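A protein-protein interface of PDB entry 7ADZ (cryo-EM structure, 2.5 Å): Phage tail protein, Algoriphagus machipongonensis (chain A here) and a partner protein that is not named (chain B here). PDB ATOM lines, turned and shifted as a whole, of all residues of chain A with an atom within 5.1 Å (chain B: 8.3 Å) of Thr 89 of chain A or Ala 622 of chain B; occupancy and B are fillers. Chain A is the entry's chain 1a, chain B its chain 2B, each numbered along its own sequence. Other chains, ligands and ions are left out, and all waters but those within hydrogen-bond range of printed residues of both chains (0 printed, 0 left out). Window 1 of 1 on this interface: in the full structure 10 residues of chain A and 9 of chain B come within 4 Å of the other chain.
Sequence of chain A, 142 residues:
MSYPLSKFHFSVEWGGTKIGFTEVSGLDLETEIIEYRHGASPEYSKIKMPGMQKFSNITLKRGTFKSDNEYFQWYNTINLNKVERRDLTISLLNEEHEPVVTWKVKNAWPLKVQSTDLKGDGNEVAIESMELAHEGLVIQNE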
ATOM      1  N   SER A  11     -24.948  19.112  -8.784  1.00  0.00           N
ATOM      2  CA  SER A  11     -24.853  19.815 -10.057  1.00  0.00           C
ATOM      3  C   SER A  11     -26.141  19.630 -10.848  1.00  0.00           C
ATOM      4  O   SER A  11     -26.893  18.680 -10.630  1.00  0.00           O
ATOM      5  CB  SER A  11     -23.652  19.335 -10.882  1.00  0.00           C
ATOM      6  OG  SER A  11     -23.781  17.977 -11.253  1.00  0.00           O
ATOM      7  N   VAL A  12     -26.395  20.559 -11.772  1.00  0.00           N
ATOM      8  CA  VAL A  12     -27.618  20.581 -12.574  1.00  0.00           C
ATOM      9  C   VAL A  12     -27.237  20.836 -14.027  1.00  0.00           C
ATOM     10  O   VAL A  12     -26.588  21.842 -14.331  1.00  0.00           O
ATOM     11  CB  VAL A  12     -28.612  21.659 -12.093  1.00  0.00           C
ATOM     12  CG1 VAL A  12     -29.733  21.856 -13.105  1.00  0.00           C
ATOM     13  CG2 VAL A  12     -29.192  21.314 -10.737  1.00  0.00           C
ATOM     14  N   GLU A  13     -27.652  19.941 -14.923  1.00  0.00           N
ATOM     15  CA  GLU A  13     -27.484  20.134 -16.365  1.00  0.00           C
ATOM     16  C   GLU A  13     -28.828  20.543 -16.956  1.00  0.00           C
ATOM     17  O   GLU A  13     -29.760  19.742 -17.020  1.00  0.00           O
ATOM     18  CB  GLU A  13     -26.948  18.873 -17.030  1.00  0.00           C
ATOM     19  CG  GLU A  13     -25.551  18.495 -16.595  1.00  0.00           C
ATOM     20  CD  GLU A  13     -24.472  19.240 -17.353  1.00  0.00           C
ATOM     21  OE1 GLU A  13     -24.799  20.005 -18.286  1.00  0.00           O
ATOM     22  OE2 GLU A  13     -23.285  19.063 -17.014  1.00  0.00           O
ATOM     23  N   ASP A  87     -34.355  18.528 -21.595  1.00  0.00           N
ATOM     24  CA  ASP A  87     -34.089  17.471 -20.629  1.00  0.00           C
ATOM     25  C   ASP A  87     -33.256  18.036 -19.487  1.00  0.00           C
ATOM     26  O   ASP A  87     -32.413  18.912 -19.697  1.00  0.00           O
ATOM     27  CB  ASP A  87     -33.367  16.289 -21.274  1.00  0.00           C
ATOM     28  CG  ASP A  87     -34.169  15.651 -22.386  1.00  0.00           C
ATOM     29  OD1 ASP A  87     -35.394  15.479 -22.219  1.00  0.00           O
ATOM     30  OD2 ASP A  87     -33.576  15.313 -23.431  1.00  0.00           O
ATOM     31  N   LEU A  88     -33.504  17.538 -18.285  1.00  0.00           N
ATOM     32  CA  LEU A  88     -32.918  18.065 -17.062  1.00  0.00           C
ATOM     33  C   LEU A  88     -32.302  16.909 -16.284  1.00  0.00           C
ATOM     34  O   LEU A  88     -32.977  15.907 -16.032  1.00  0.00           O
ATOM     35  CB  LEU A  88     -33.994  18.781 -16.246  1.00  0.00           C
ATOM     36  CG  LEU A  88     -33.680  19.618 -15.014  1.00  0.00           C
ATOM     37  CD1 LEU A  88     -32.996  20.893 -15.405  1.00  0.00           C
ATOM     38  CD2 LEU A  88     -34.964  19.917 -14.273  1.00  0.00           C
ATOM     39  N   THR A  89     -31.031  17.040 -15.910  1.00  0.00           N
ATOM     40  CA  THR A  89     -30.315  15.998 -15.181  1.00  0.00           C
ATOM     41  C   THR A  89     -29.676  16.590 -13.932  1.00  0.00           C
ATOM     42  O   THR A  89     -28.824  17.476 -14.027  1.00  0.00           O
ATOM     43  CB  THR A  89     -29.248  15.333 -16.061  1.00  0.00           C
ATOM     44  OG1 THR A  89     -29.880  14.629 -17.133  1.00  0.00           O
ATOM     45  CG2 THR A  89     -28.427  14.346 -15.265  1.00  0.00           C
ATOM     46  N   ILE A  90     -30.075  16.080 -12.770  1.00  0.00           N
ATOM     47  CA  ILE A  90     -29.647  16.585 -11.471  1.00  0.00           C
ATOM     48  C   ILE A  90     -28.952  15.452 -10.729  1.00  0.00           C
ATOM     49  O   ILE A  90     -29.531  14.375 -10.561  1.00  0.00           O
ATOM     50  CB  ILE A  90     -30.844  17.130 -10.665  1.00  0.00           C
ATOM     51  CG1 ILE A  90     -31.527  18.265 -11.436  1.00  0.00           C
ATOM     52  CG2 ILE A  90     -30.412  17.604  -9.292  1.00  0.00           C
ATOM     53  CD1 ILE A  90     -32.896  18.632 -10.935  1.00  0.00           C
ATOM     54  N   SER A  91     -27.715  15.688 -10.291  1.00  0.00           N
ATOM     55  CA  SER A  91     -26.885  14.644  -9.697  1.00  0.00           C
ATOM     56  C   SER A  91     -26.395  15.054  -8.317  1.00  0.00           C
ATOM     57  O   SER A  91     -26.116  16.228  -8.076  1.00  0.00           O
ATOM     58  CB  SER A  91     -25.674  14.321 -10.581  1.00  0.00           C
ATOM     59  OG  SER A  91     -26.063  13.712 -11.796  1.00  0.00           O
ATOM     60  N   THR A 102     -29.068  10.217  -9.273  1.00  0.00           N
ATOM     61  CA  THR A 102     -29.424  11.063 -10.401  1.00  0.00           C
ATOM     62  C   THR A 102     -30.939  11.099 -10.574  1.00  0.00           C
ATOM     63  O   THR A 102     -31.612  10.070 -10.514  1.00  0.00           O
ATOM     64  CB  THR A 102     -28.739  10.563 -11.693  1.00  0.00           C
ATOM     65  OG1 THR A 102     -27.325  10.495 -11.490  1.00  0.00           O
ATOM     66  CG2 THR A 102     -29.002  11.491 -12.864  1.00  0.00           C
ATOM     67  N   TRP A 103     -31.466  12.305 -10.783  1.00  0.00           N
ATOM     68  CA  TRP A 103     -32.871  12.534 -11.101  1.00  0.00           C
ATOM     69  C   TRP A 103     -32.961  12.954 -12.561  1.00  0.00           C
ATOM     70  O   TRP A 103     -32.299  13.909 -12.974  1.00  0.00           O
ATOM     71  CB  TRP A 103     -33.474  13.603 -10.180  1.00  0.00           C
ATOM     72  CG  TRP A 103     -33.545  13.187  -8.732  1.00  0.00           C
ATOM     73  CD1 TRP A 103     -34.575  12.545  -8.117  1.00  0.00           C
ATOM     74  CD2 TRP A 103     -32.539  13.379  -7.727  1.00  0.00           C
ATOM     75  NE1 TRP A 103     -34.277  12.320  -6.800  1.00  0.00           N
ATOM     76  CE2 TRP A 103     -33.032  12.820  -6.534  1.00  0.00           C
ATOM     77  CE3 TRP A 103     -31.270  13.962  -7.724  1.00  0.00           C
ATOM     78  CZ2 TRP A 103     -32.304  12.837  -5.345  1.00  0.00           C
ATOM     79  CZ3 TRP A 103     -30.550  13.977  -6.548  1.00  0.00           C
ATOM     80  CH2 TRP A 103     -31.066  13.415  -5.374  1.00  0.00           C
ATOM     81  N   LYS A 104     -33.747  12.223 -13.349  1.00  0.00           N
ATOM     82  CA  LYS A 104     -33.838  12.438 -14.791  1.00  0.00           C
ATOM     83  C   LYS A 104     -35.233  12.931 -15.153  1.00  0.00           C
ATOM     84  O   LYS A 104     -36.225  12.247 -14.894  1.00  0.00           O
ATOM     85  CB  LYS A 104     -33.497  11.157 -15.548  1.00  0.00           C
ATOM     86  CG  LYS A 104     -32.021  10.818 -15.508  1.00  0.00           C
ATOM     87  CD  LYS A 104     -31.741   9.469 -16.127  1.00  0.00           C
ATOM     88  CE  LYS A 104     -32.136   8.351 -15.184  1.00  0.00           C
ATOM     89  NZ  LYS A 104     -31.822   7.004 -15.729  1.00  0.00           N
ATOM     90  N   ALA B 603     -27.811  12.871 -30.759  1.00  0.00           N
ATOM     91  CA  ALA B 603     -27.636  12.893 -29.311  1.00  0.00           C
ATOM     92  C   ALA B 603     -26.203  12.565 -28.866  1.00  0.00           C
ATOM     93  O   ALA B 603     -25.745  13.097 -27.855  1.00  0.00           O
ATOM     94  CB  ALA B 603     -28.587  11.906 -28.642  1.00  0.00           C
ATOM     95  N   GLY B 614     -17.955   9.457 -15.903  1.00  0.00           N
ATOM     96  CA  GLY B 614     -19.302   9.229 -15.398  1.00  0.00           C
ATOM     97  C   GLY B 614     -20.298  10.332 -15.676  1.00  0.00           C
ATOM     98  O   GLY B 614     -21.473  10.058 -15.905  1.00  0.00           O
ATOM     99  N   ASN B 615     -19.860  11.579 -15.685  1.00  0.00           N
ATOM    100  CA  ASN B 615     -20.799  12.655 -15.935  1.00  0.00           C
ATOM    101  C   ASN B 615     -21.359  12.606 -17.356  1.00  0.00           C
ATOM    102  O   ASN B 615     -22.531  12.939 -17.582  1.00  0.00           O
ATOM    103  CB  ASN B 615     -20.124  13.972 -15.675  1.00  0.00           C
ATOM    104  CG  ASN B 615     -19.888  14.195 -14.230  1.00  0.00           C
ATOM    105  OD1 ASN B 615     -20.563  13.637 -13.363  1.00  0.00           O
ATOM    106  ND2 ASN B 615     -18.917  14.998 -13.935  1.00  0.00           N
ATOM    107  N   THR B 616     -20.528  12.177 -18.306  1.00  0.00           N
ATOM    108  CA  THR B 616     -20.902  12.096 -19.697  1.00  0.00           C
ATOM    109  C   THR B 616     -21.807  10.915 -19.875  1.00  0.00           C
ATOM    110  O   THR B 616     -22.879  11.009 -20.467  1.00  0.00           O
ATOM    111  CB  THR B 616     -19.657  11.961 -20.607  1.00  0.00           C
ATOM    112  OG1 THR B 616     -18.817  13.126 -20.455  1.00  0.00           O
ATOM    113  CG2 THR B 616     -20.080  11.817 -22.058  1.00  0.00           C
ATOM    114  N   TRP B 617     -21.412   9.787 -19.311  1.00  0.00           N
ATOM    115  CA  TRP B 617     -22.170   8.569 -19.508  1.00  0.00           C
ATOM    116  C   TRP B 617     -23.606   8.757 -19.026  1.00  0.00           C
ATOM    117  O   TRP B 617     -24.554   8.360 -19.712  1.00  0.00           O
ATOM    118  CB  TRP B 617     -21.468   7.431 -18.793  1.00  0.00           C
ATOM    119  CG  TRP B 617     -20.050   7.273 -19.268  1.00  0.00           C
ATOM    120  CD1 TRP B 617     -19.518   7.710 -20.438  1.00  0.00           C
ATOM    121  CD2 TRP B 617     -18.965   6.685 -18.553  1.00  0.00           C
ATOM    122  NE1 TRP B 617     -18.206   7.447 -20.474  1.00  0.00           N
ATOM    123  CE2 TRP B 617     -17.847   6.827 -19.338  1.00  0.00           C
ATOM    124  CE3 TRP B 617     -18.850   6.074 -17.318  1.00  0.00           C
ATOM    125  CZ2 TRP B 617     -16.630   6.388 -18.941  1.00  0.00           C
ATOM    126  CZ3 TRP B 617     -17.615   5.633 -16.917  1.00  0.00           C
ATOM    127  CH2 TRP B 617     -16.534   5.789 -17.712  1.00  0.00           C
ATOM    128  N   VAL B 618     -23.790   9.429 -17.886  1.00  0.00           N
ATOM    129  CA  VAL B 618     -25.133   9.675 -17.393  1.00  0.00           C
ATOM    130  C   VAL B 618     -25.936  10.568 -18.335  1.00  0.00           C
ATOM    131  O   VAL B 618     -27.098  10.264 -18.619  1.00  0.00           O
ATOM    132  CB  VAL B 618     -25.093  10.286 -15.984  1.00  0.00           C
ATOM    133  CG1 VAL B 618     -26.478  10.736 -15.551  1.00  0.00           C
ATOM    134  CG2 VAL B 618     -24.586   9.251 -15.024  1.00  0.00           C
ATOM    135  N   ARG B 619     -25.354  11.673 -18.814  1.00  0.00           N
ATOM    136  CA  ARG B 619     -26.088  12.530 -19.732  1.00  0.00           C
ATOM    137  C   ARG B 619     -26.461  11.836 -21.034  1.00  0.00           C
ATOM    138  O   ARG B 619     -27.580  12.011 -21.521  1.00  0.00           O
ATOM    139  CB  ARG B 619     -25.298  13.770 -20.057  1.00  0.00           C
ATOM    140  CG  ARG B 619     -25.200  14.746 -18.930  1.00  0.00           C
ATOM    141  CD  ARG B 619     -24.342  15.878 -19.272  1.00  0.00           C
ATOM    142  NE  ARG B 619     -24.907  16.676 -20.348  1.00  0.00           N
ATOM    143  CZ  ARG B 619     -24.243  17.621 -21.036  1.00  0.00           C
ATOM    144  NH1 ARG B 619     -22.985  17.885 -20.755  1.00  0.00           N
ATOM    145  NH2 ARG B 619     -24.862  18.279 -21.999  1.00  0.00           N
ATOM    146  N   VAL B 620     -25.554  11.025 -21.579  1.00  0.00           N
ATOM    147  CA  VAL B 620     -25.822  10.333 -22.830  1.00  0.00           C
ATOM    148  C   VAL B 620     -26.990   9.387 -22.669  1.00  0.00           C
ATOM    149  O   VAL B 620     -27.904   9.366 -23.502  1.00  0.00           O
ATOM    150  CB  VAL B 620     -24.565   9.553 -23.294  1.00  0.00           C
ATOM    151  CG1 VAL B 620     -24.870   8.632 -24.471  1.00  0.00           C
ATOM    152  CG2 VAL B 620     -23.518  10.529 -23.723  1.00  0.00           C
ATOM    153  N   ARG B 621     -26.968   8.599 -21.605  1.00  0.00           N
ATOM    154  CA  ARG B 621     -28.043   7.675 -21.376  1.00  0.00           C
ATOM    155  C   ARG B 621     -29.382   8.376 -21.211  1.00  0.00           C
ATOM    156  O   ARG B 621     -30.372   7.952 -21.809  1.00  0.00           O
ATOM    157  CB  ARG B 621     -27.760   6.814 -20.176  1.00  0.00           C
ATOM    158  CG  ARG B 621     -28.837   5.826 -19.877  1.00  0.00           C
ATOM    159  CD  ARG B 621     -28.466   4.925 -18.821  1.00  0.00           C
ATOM    160  NE  ARG B 621     -29.597   4.161 -18.410  1.00  0.00           N
ATOM    161  CZ  ARG B 621     -29.619   3.228 -17.464  1.00  0.00           C
ATOM    162  NH1 ARG B 621     -28.532   2.888 -16.805  1.00  0.00           N
ATOM    163  NH2 ARG B 621     -30.778   2.666 -17.218  1.00  0.00           N
ATOM    164  N   ALA B 622     -29.433   9.448 -20.419  1.00  0.00           N
ATOM    165  CA  ALA B 622     -30.692  10.145 -20.204  1.00  0.00           C
ATOM    166  C   ALA B 622     -31.291  10.698 -21.495  1.00  0.00           C
ATOM    167  O   ALA B 622     -32.505  10.625 -21.698  1.00  0.00           O
ATOM    168  CB  ALA B 622     -30.474  11.278 -19.230  1.00  0.00           C
ATOM    169  N   MET B 623     -30.452  11.240 -22.383  1.00  0.00           N
ATOM    170  CA  MET B 623     -30.951  11.783 -23.640  1.00  0.00           C
ATOM    171  C   MET B 623     -31.596  10.707 -24.504  1.00  0.00           C
ATOM    172  O   MET B 623     -32.682  10.915 -25.066  1.00  0.00           O
ATOM    173  CB  MET B 623     -29.807  12.448 -24.392  1.00  0.00           C
ATOM    174  CG  MET B 623     -29.309  13.729 -23.751  1.00  0.00           C
ATOM    175  SD  MET B 623     -27.770  14.337 -24.475  1.00  0.00           S
ATOM    176  CE  MET B 623     -28.245  14.934 -26.068  1.00  0.00           C
ATOM    177  N   ILE B 624     -30.937   9.556 -24.604  1.00  0.00           N
ATOM    178  CA  ILE B 624     -31.440   8.473 -25.424  1.00  0.00           C
ATOM    179  C   ILE B 624     -32.736   7.914 -24.862  1.00  0.00           C
ATOM    180  O   ILE B 624     -33.677   7.670 -25.625  1.00  0.00           O
ATOM    181  CB  ILE B 624     -30.404   7.365 -25.596  1.00  0.00           C
ATOM    182  CG1 ILE B 624     -29.218   7.922 -26.392  1.00  0.00           C
ATOM    183  CG2 ILE B 624     -31.053   6.172 -26.360  1.00  0.00           C
ATOM    184  CD1 ILE B 624     -27.996   7.060 -26.389  1.00  0.00           C
ATOM    185  N   GLU B 625     -32.785   7.656 -23.548  1.00  0.00           N
ATOM    186  CA  GLU B 625     -34.006   7.114 -22.983  1.00  0.00           C
ATOM    187  C   GLU B 625     -35.181   8.062 -23.157  1.00  0.00           C
ATOM    188  O   GLU B 625     -36.267   7.619 -23.518  1.00  0.00           O
ATOM    189  CB  GLU B 625     -33.850   6.774 -21.506  1.00  0.00           C
ATOM    190  CG  GLU B 625     -32.983   5.556 -21.191  1.00  0.00           C
ATOM    191  CD  GLU B 625     -32.869   5.317 -19.705  1.00  0.00           C
ATOM    192  OE1 GLU B 625     -33.218   6.204 -18.971  1.00  0.00           O
ATOM    193  OE2 GLU B 625     -32.456   4.246 -19.293  1.00  0.00           O
ATOM    194  N   ASN B 626     -34.995   9.378 -23.002  1.00  0.00           N
ATOM    195  CA  ASN B 626     -36.153  10.244 -23.161  1.00  0.00           C
ATOM    196  C   ASN B 626     -36.736  10.133 -24.568  1.00  0.00           C
ATOM    197  O   ASN B 626     -37.960  10.064 -24.736  1.00  0.00           O
ATOM    198  CB  ASN B 626     -35.791  11.664 -22.827  1.00  0.00           C
ATOM    199  CG  ASN B 626     -35.607  11.867 -21.352  1.00  0.00           C
ATOM    200  OD1 ASN B 626     -36.072  11.083 -20.523  1.00  0.00           O
ATOM    201  ND2 ASN B 626     -34.930  12.914 -21.004  1.00  0.00           N
ATOM    202  N   PHE B 627     -35.873  10.044 -25.580  1.00  0.00           N
ATOM    203  CA  PHE B 627     -36.341   9.865 -26.946  1.00  0.00           C
ATOM    204  C   PHE B 627     -37.173   8.597 -27.090  1.00  0.00           C
ATOM    205  O   PHE B 627     -38.279   8.620 -27.649  1.00  0.00           O
ATOM    206  CB  PHE B 627     -35.161   9.841 -27.924  1.00  0.00           C
ATOM    207  CG  PHE B 627     -35.527   9.444 -29.331  1.00  0.00           C
ATOM    208  CD1 PHE B 627     -36.193  10.301 -30.171  1.00  0.00           C
ATOM    209  CD2 PHE B 627     -35.187   8.191 -29.808  1.00  0.00           C
ATOM    210  CE1 PHE B 627     -36.526   9.910 -31.446  1.00  0.00           C
ATOM    211  CE2 PHE B 627     -35.515   7.805 -31.078  1.00  0.00           C
ATOM    212  CZ  PHE B 627     -36.188   8.664 -31.893  1.00  0.00           C
ATOM    213  N   LEU B 628     -36.636   7.485 -26.605  1.00  0.00           N
ATOM    214  CA  LEU B 628     -37.318   6.214 -26.741  1.00  0.00           C
ATOM    215  C   LEU B 628     -38.635   6.159 -25.965  1.00  0.00           C
ATOM    216  O   LEU B 628     -39.587   5.519 -26.426  1.00  0.00           O
ATOM    217  CB  LEU B 628     -36.377   5.088 -26.345  1.00  0.00           C
ATOM    218  CG  LEU B 628     -35.135   4.879 -27.276  1.00  0.00           C
ATOM    219  CD1 LEU B 628     -34.259   3.816 -26.676  1.00  0.00           C
ATOM    220  CD2 LEU B 628     -35.562   4.507 -28.685  1.00  0.00           C
ATOM    221  N   ILE B 629     -38.722   6.829 -24.814  1.00  0.00           N
ATOM    222  CA  ILE B 629     -39.965   6.850 -24.052  1.00  0.00           C
ATOM    223  C   ILE B 629     -41.048   7.514 -24.870  1.00  0.00           C
ATOM    224  O   ILE B 629     -42.180   7.033 -24.893  1.00  0.00           O
ATOM    225  CB  ILE B 629     -39.848   7.553 -22.692  1.00  0.00           C
ATOM    226  CG1 ILE B 629     -38.955   6.736 -21.793  1.00  0.00           C
ATOM    227  CG2 ILE B 629     -41.256   7.708 -22.066  1.00  0.00           C
ATOM    228  CD1 ILE B 629     -38.489   7.411 -20.549  1.00  0.00           C
ATOM    229  N   VAL B 648     -31.079   0.724 -22.713  1.00  0.00           N
ATOM    230  CA  VAL B 648     -29.872   1.456 -23.091  1.00  0.00           C
ATOM    231  C   VAL B 648     -28.755   1.191 -22.074  1.00  0.00           C
ATOM    232  O   VAL B 648     -28.996   1.299 -20.878  1.00  0.00           O
ATOM    233  CB  VAL B 648     -30.161   2.983 -23.141  1.00  0.00           C
ATOM    234  CG1 VAL B 648     -28.900   3.776 -23.560  1.00  0.00           C
ATOM    235  CG2 VAL B 648     -31.311   3.272 -24.090  1.00  0.00           C
ATOM    236  N   VAL B 650     -24.620   2.265 -21.155  1.00  0.00           N
ATOM    237  CA  VAL B 650     -23.397   3.016 -21.451  1.00  0.00           C
ATOM    238  C   VAL B 650     -22.487   3.032 -20.224  1.00  0.00           C
ATOM    239  O   VAL B 650     -22.943   3.447 -19.164  1.00  0.00           O
ATOM    240  CB  VAL B 650     -23.717   4.503 -21.787  1.00  0.00           C
ATOM    241  CG1 VAL B 650     -22.417   5.271 -22.185  1.00  0.00           C
ATOM    242  CG2 VAL B 650     -24.750   4.585 -22.857  1.00  0.00           C
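Of the printed residues of chain B, Glu 13 of chain A touches Arg 619 (3.7 Å).
Of the printed residues of chain B, Asp 87 of chain A touches Asn 626 (2.9 Å).
Printed residues of chain B within 4 Å of Thr 89 of chain A: Ala 622 (3.997 Å).
Of the printed residues of chain B, Thr 102 of chain A touches Val 618 (3.8 Å).
Printed residues of chain B within 4 Å of Lys 104 of chain A: Ala 622 (3.8 Å) and Glu 625 (3.6 Å).
Of the printed residues of chain A, Ala 622 of chain B touches Thr 89 and Lys 104.
The nearest printed residue of chain B that does not touch Thr 89 of chain A is Val 618 of chain B (4.1 Å).
N of Glu 13 of chain A lies within hydrogen-bond range of O of Thr 89 of chain A, 2.9 Å away.
The side-chain hydroxyl (OG1) of Thr 102 of chain A lies within hydrogen-bond range of the side-chain hydroxyl (OG) of Ser 91 of chain A (3.5 Å).
The guanidinium group (NE) of Arg 621 of chain B is in salt-bridge range of the side-chain carboxylate (OE2) of Glu 625 of chain B (3.0 Å).
ND2 of Asn 626 of chain B lies close to O of Ala 622 of chain B (3.4 Å).
OE1 of Glu 13 of chain A lies within salt-bridge range of NH1 of Arg 619 of chain B (3.7 Å).
ND2 of Asn 626 of chain B is in hydrogen-bond range of OD1 of Asp 87 of chain A (2.9 Å).
NZ of Lys 104 of chain A is in salt-bridge range of OE1 of Glu 625 of chain B (3.6 Å).
Of the 19 printed residues of chain B, 5 touch a printed residue of chain A.
Hydrophobic or aromatic side chains of chain B within 4 Å of the printed part of chain A: Val 618 and Ala 622.
Of the 11 printed residues of chain A, 5 touch a printed residue of chain B.
Among the printed residues, pairs that only touch across the chains: Thr 102 of chain A with Val 618 of chain B (3.8 Å), Lys 104 of chain A with Ala 622 of chain B (3.8 Å) and Thr 89 of chain A with Ala 622 of chain B (3.997 Å).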
